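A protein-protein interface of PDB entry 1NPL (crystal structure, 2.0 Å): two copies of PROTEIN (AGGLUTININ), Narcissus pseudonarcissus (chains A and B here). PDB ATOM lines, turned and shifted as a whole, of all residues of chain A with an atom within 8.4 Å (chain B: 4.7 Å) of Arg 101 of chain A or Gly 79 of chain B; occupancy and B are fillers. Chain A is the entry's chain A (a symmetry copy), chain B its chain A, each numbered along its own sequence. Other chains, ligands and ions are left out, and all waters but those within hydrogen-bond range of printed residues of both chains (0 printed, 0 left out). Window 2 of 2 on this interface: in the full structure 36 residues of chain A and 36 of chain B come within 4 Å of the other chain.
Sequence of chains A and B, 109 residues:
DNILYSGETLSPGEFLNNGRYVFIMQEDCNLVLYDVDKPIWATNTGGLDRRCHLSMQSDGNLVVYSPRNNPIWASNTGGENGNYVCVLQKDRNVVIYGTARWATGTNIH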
ATOM      1  N   ASN A  83     -17.903  28.407  21.200  1.00  0.00           N
ATOM      2  CA  ASN A  83     -17.876  29.860  20.974  1.00  0.00           C
ATOM      3  C   ASN A  83     -19.221  30.347  21.500  1.00  0.00           C
ATOM      4  O   ASN A  83     -20.230  29.827  21.031  1.00  0.00           O
ATOM      5  CB  ASN A  83     -17.669  30.241  19.505  1.00  0.00           C
ATOM      6  CG  ASN A  83     -16.205  30.028  19.103  1.00  0.00           C
ATOM      7  OD1 ASN A  83     -15.268  30.787  19.415  1.00  0.00           O
ATOM      8  ND2 ASN A  83     -16.041  28.980  18.369  1.00  0.00           N
ATOM      9  N   GLY A  98     -25.175  30.350  22.785  1.00  0.00           N
ATOM     10  CA  GLY A  98     -24.120  29.488  22.120  1.00  0.00           C
ATOM     11  C   GLY A  98     -24.515  27.997  22.295  1.00  0.00           C
ATOM     12  O   GLY A  98     -25.532  27.791  22.941  1.00  0.00           O
ATOM     13  N   THR A  99     -23.802  27.056  21.655  1.00  0.00           N
ATOM     14  CA  THR A  99     -22.620  27.396  20.858  1.00  0.00           C
ATOM     15  C   THR A  99     -22.937  27.856  19.451  1.00  0.00           C
ATOM     16  O   THR A  99     -24.101  27.969  19.053  1.00  0.00           O
ATOM     17  CB  THR A  99     -21.610  26.223  20.850  1.00  0.00           C
ATOM     18  OG1 THR A  99     -22.247  25.079  20.227  1.00  0.00           O
ATOM     19  CG2 THR A  99     -21.411  25.744  22.295  1.00  0.00           C
ATOM     20  N   ALA A 100     -21.903  28.174  18.632  1.00  0.00           N
ATOM     21  CA  ALA A 100     -22.104  28.488  17.235  1.00  0.00           C
ATOM     22  C   ALA A 100     -22.677  27.304  16.452  1.00  0.00           C
ATOM     23  O   ALA A 100     -22.031  26.259  16.507  1.00  0.00           O
ATOM     24  CB  ALA A 100     -20.760  28.875  16.563  1.00  0.00           C
ATOM     25  N   ARG A 101     -23.795  27.437  15.754  1.00  0.00           N
ATOM     26  CA  ARG A 101     -24.367  26.393  14.940  1.00  0.00           C
ATOM     27  C   ARG A 101     -23.970  26.426  13.480  1.00  0.00           C
ATOM     28  O   ARG A 101     -24.067  25.391  12.851  1.00  0.00           O
ATOM     29  CB  ARG A 101     -25.915  26.435  14.992  1.00  0.00           C
ATOM     30  CG  ARG A 101     -26.484  26.571  16.409  1.00  0.00           C
ATOM     31  CD  ARG A 101     -28.013  26.510  16.338  1.00  0.00           C
ATOM     32  NE  ARG A 101     -28.461  25.327  15.653  1.00  0.00           N
ATOM     33  CZ  ARG A 101     -29.463  24.518  15.443  1.00  0.00           C
ATOM     34  NH1 ARG A 101     -30.690  24.547  15.936  1.00  0.00           N
ATOM     35  NH2 ARG A 101     -29.197  23.491  14.599  1.00  0.00           N
ATOM     36  N   TRP A 102     -23.696  27.591  12.895  1.00  0.00           N
ATOM     37  CA  TRP A 102     -23.402  27.749  11.458  1.00  0.00           C
ATOM     38  C   TRP A 102     -22.596  29.036  11.257  1.00  0.00           C
ATOM     39  O   TRP A 102     -22.805  29.935  12.111  1.00  0.00           O
ATOM     40  CB  TRP A 102     -24.656  27.847  10.662  1.00  0.00           C
ATOM     41  CG  TRP A 102     -24.534  28.091   9.187  1.00  0.00           C
ATOM     42  CD1 TRP A 102     -24.303  27.147   8.215  1.00  0.00           C
ATOM     43  CD2 TRP A 102     -24.592  29.375   8.547  1.00  0.00           C
ATOM     44  NE1 TRP A 102     -24.255  27.785   6.996  1.00  0.00           N
ATOM     45  CE2 TRP A 102     -24.421  29.139   7.157  1.00  0.00           C
ATOM     46  CE3 TRP A 102     -24.782  30.692   9.007  1.00  0.00           C
ATOM     47  CZ2 TRP A 102     -24.417  30.178   6.226  1.00  0.00           C
ATOM     48  CZ3 TRP A 102     -24.802  31.736   8.086  1.00  0.00           C
ATOM     49  CH2 TRP A 102     -24.590  31.458   6.708  1.00  0.00           C
ATOM     50  N   ALA A 103     -21.702  29.104  10.284  1.00  0.00           N
ATOM     51  CA  ALA A 103     -20.934  30.321  10.026  1.00  0.00           C
ATOM     52  C   ALA A 103     -20.653  30.424   8.530  1.00  0.00           C
ATOM     53  O   ALA A 103     -20.556  29.355   7.886  1.00  0.00           O
ATOM     54  CB  ALA A 103     -19.635  30.350  10.811  1.00  0.00           C
ATOM     55  N   THR A 104     -20.627  31.620   7.944  1.00  0.00           N
ATOM     56  CA  THR A 104     -20.074  31.732   6.580  1.00  0.00           C
ATOM     57  C   THR A 104     -18.602  31.343   6.493  1.00  0.00           C
ATOM     58  O   THR A 104     -18.059  31.035   5.390  1.00  0.00           O
ATOM     59  CB  THR A 104     -20.271  33.162   6.048  1.00  0.00           C
ATOM     60  OG1 THR A 104     -19.708  34.084   6.971  1.00  0.00           O
ATOM     61  CG2 THR A 104     -21.753  33.545   5.916  1.00  0.00           C
ATOM     62  N   ASP B  59     -36.768  27.765  15.024  1.00  0.00           N
ATOM     63  CA  ASP B  59     -36.151  26.420  15.099  1.00  0.00           C
ATOM     64  C   ASP B  59     -34.656  26.542  14.900  1.00  0.00           C
ATOM     65  O   ASP B  59     -33.938  25.526  14.912  1.00  0.00           O
ATOM     66  CB  ASP B  59     -36.758  25.391  14.156  1.00  0.00           C
ATOM     67  CG  ASP B  59     -36.679  25.662  12.666  1.00  0.00           C
ATOM     68  OD1 ASP B  59     -36.191  26.736  12.269  1.00  0.00           O
ATOM     69  OD2 ASP B  59     -37.158  24.839  11.823  1.00  0.00           O
ATOM     70  N   GLY B  60     -34.131  27.740  14.649  1.00  0.00           N
ATOM     71  CA  GLY B  60     -32.686  27.893  14.508  1.00  0.00           C
ATOM     72  C   GLY B  60     -32.175  27.896  13.072  1.00  0.00           C
ATOM     73  O   GLY B  60     -30.979  28.099  12.841  1.00  0.00           O
ATOM     74  N   THR B  77     -29.821  24.310   9.705  1.00  0.00           N
ATOM     75  CA  THR B  77     -29.486  24.213  11.147  1.00  0.00           C
ATOM     76  C   THR B  77     -30.777  24.151  11.951  1.00  0.00           C
ATOM     77  O   THR B  77     -30.881  24.625  13.082  1.00  0.00           O
ATOM     78  CB  THR B  77     -28.609  25.398  11.574  1.00  0.00           C
ATOM     79  OG1 THR B  77     -29.204  26.632  11.088  1.00  0.00           O
ATOM     80  CG2 THR B  77     -27.268  25.221  10.905  1.00  0.00           C
ATOM     81  N   GLY B  78     -31.817  23.689  11.265  1.00  0.00           N
ATOM     82  CA  GLY B  78     -33.160  23.649  11.869  1.00  0.00           C
ATOM     83  C   GLY B  78     -33.097  22.564  12.940  1.00  0.00           C
ATOM     84  O   GLY B  78     -32.589  21.470  12.702  1.00  0.00           O
ATOM     85  N   GLY B  79     -33.510  22.911  14.152  1.00  0.00           N
ATOM     86  CA  GLY B  79     -33.294  21.992  15.263  1.00  0.00           C
ATOM     87  C   GLY B  79     -34.207  22.376  16.418  1.00  0.00           C
ATOM     88  O   GLY B  79     -35.405  22.598  16.207  1.00  0.00           O
ATOM     89  N   GLU B  80     -33.664  22.466  17.640  1.00  0.00           N
ATOM     90  CA  GLU B  80     -34.620  22.730  18.707  1.00  0.00           C
ATOM     91  C   GLU B  80     -35.146  24.168  18.748  1.00  0.00           C
ATOM     92  O   GLU B  80     -34.483  25.152  18.477  1.00  0.00           O
ATOM     93  CB  GLU B  80     -34.199  22.309  20.105  1.00  0.00           C
ATOM     94  CG  GLU B  80     -35.433  22.053  20.971  1.00  0.00           C
ATOM     95  CD  GLU B  80     -36.565  21.301  20.302  1.00  0.00           C
ATOM     96  OE1 GLU B  80     -36.355  20.206  19.730  1.00  0.00           O
ATOM     97  OE2 GLU B  80     -37.708  21.825  20.327  1.00  0.00           O
ATOM     98  N   ASN B  81     -36.437  24.200  19.085  1.00  0.00           N
ATOM     99  CA  ASN B  81     -37.187  25.413  19.278  1.00  0.00           C
ATOM    100  C   ASN B  81     -36.613  26.228  20.443  1.00  0.00           C
ATOM    101  O   ASN B  81     -36.335  25.685  21.520  1.00  0.00           O
ATOM    102  CB  ASN B  81     -38.660  25.144  19.522  1.00  0.00           C
ATOM    103  CG  ASN B  81     -39.534  26.308  19.873  1.00  0.00           C
ATOM    104  OD1 ASN B  81     -40.040  26.440  20.994  1.00  0.00           O
ATOM    105  ND2 ASN B  81     -39.833  27.251  18.975  1.00  0.00           N
ATOM    106  N   TYR B  84     -32.706  32.354  19.030  1.00  0.00           N
ATOM    107  CA  TYR B  84     -31.374  32.365  18.400  1.00  0.00           C
ATOM    108  C   TYR B  84     -31.046  33.797  17.966  1.00  0.00           C
ATOM    109  O   TYR B  84     -31.981  34.615  17.850  1.00  0.00           O
ATOM    110  CB  TYR B  84     -31.337  31.413  17.170  1.00  0.00           C
ATOM    111  CG  TYR B  84     -31.623  29.944  17.423  1.00  0.00           C
ATOM    112  CD1 TYR B  84     -32.928  29.490  17.607  1.00  0.00           C
ATOM    113  CD2 TYR B  84     -30.597  29.020  17.523  1.00  0.00           C
ATOM    114  CE1 TYR B  84     -33.213  28.152  17.869  1.00  0.00           C
ATOM    115  CE2 TYR B  84     -30.844  27.660  17.756  1.00  0.00           C
ATOM    116  CZ  TYR B  84     -32.157  27.246  17.912  1.00  0.00           C
ATOM    117  OH  TYR B  84     -32.429  25.901  18.096  1.00  0.00           O
ATOM    118  N   ILE B  96     -24.467  32.005  13.330  1.00  0.00           N
ATOM    119  CA  ILE B  96     -25.701  31.750  14.100  1.00  0.00           C
ATOM    120  C   ILE B  96     -25.362  31.139  15.456  1.00  0.00           C
ATOM    121  O   ILE B  96     -24.655  30.090  15.528  1.00  0.00           O
ATOM    122  CB  ILE B  96     -26.716  30.832  13.376  1.00  0.00           C
ATOM    123  CG1 ILE B  96     -27.222  31.414  12.037  1.00  0.00           C
ATOM    124  CG2 ILE B  96     -27.961  30.501  14.212  1.00  0.00           C
ATOM    125  CD1 ILE B  96     -27.785  30.288  11.161  1.00  0.00           C
ATOM    126  N   GLY B  98     -27.127  29.825  19.320  1.00  0.00           N
ATOM    127  CA  GLY B  98     -28.317  29.585  20.228  1.00  0.00           C
ATOM    128  C   GLY B  98     -28.286  28.110  20.708  1.00  0.00           C
ATOM    129  O   GLY B  98     -27.379  27.425  20.258  1.00  0.00           O
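Gly 98 of chain B touches its own counterpart, Gly 98 of chain A.
Of the 10 pairs that touch across the chains among the printed residues, 1 has its exchanged pair printed and touching as well.
The guanidinium group (NH1) of Arg 101 of chain A sits at hydrogen-bond distance from the side-chain hydroxyl (OH) of Tyr 84 of chain B, 3.1 Å away.
The backbone carbonyl oxygen of Trp 102 of chain A sits at hydrogen-bond distance from the backbone NH of Ile 96 of chain B (2.9 Å).
The backbone carbonyl oxygen (O) of Gly 98 of chain A sits close to the backbone carbonyl oxygen (O) of Gly 98 of chain B (3.3 Å).
The backbone carbonyl oxygen of Ile 96 of chain B sits at hydrogen-bond distance from the backbone NH of Arg 101 of chain A, at 2.8 Å.
O of Thr 77 of chain B sits at hydrogen-bond distance from NH2 of Arg 101 of chain A (2.5 Å).
Printed residues of chain B within 4 Å of Arg 101 of chain A: Asp 59, Thr 77, Gly 79, Tyr 84 and Ile 96.
Of the printed residues of chain A, Gly 79 of chain B touches Arg 101 (3.7 Å).
Of the printed residues of chain A, Ile 96 of chain B touches Ala 100 (3.5 Å), Arg 101 (2.8 Å) and Trp 102 (2.9 Å).
Of the printed residues of chain A, Gly 98 of chain B touches Gly 98 (3.3 Å) and Thr 99 (3.5 Å).
The nearest printed residue of chain A that does not touch Gly 98 of chain B is Arg 101 of chain A (4.04 Å).
Hydrophobic or aromatic side chains of chain B that line the printed part of chain A: Tyr 84 and Ile 96.
Along chain B the printed residues that touch a printed residue of chain A span positions 59 to 98.
Hydrophobic or aromatic side chains of chain A within 4 Å of the printed part of chain B: Trp 102.
Along chain A the printed residues that touch a printed residue of chain B span positions 98 to 102.
O of Thr 99 of chain A touches O of Gly 98 of chain B, at 3.5 Å.
Ile 96 of chain B touches Ala 100 of chain A.
Arg 101 of chain A touches Asp 59 of chain B.
NH1 of Arg 101 of chain A touches CA of Gly 79 of chain B, 3.7 Å away.
Trp 102 of chain A touches Thr 77 of chain B (CB to CG2, 3.7 Å).
The side-chain hydroxyl (OG1) of Thr 77 of chain B is in hydrogen-bond range of the backbone carbonyl oxygen (O) of Gly 60 of chain B (2.9 Å).
The backbone carbonyl oxygen of Asn 83 of chain A lies within hydrogen-bond range of the backbone NH of Ala 100 of chain A, at 3.4 Å.
The backbone NH (N) of Gly 79 of chain B lies within hydrogen-bond range of the backbone carbonyl oxygen (O) of Asp 59 of chain B (2.8 Å).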
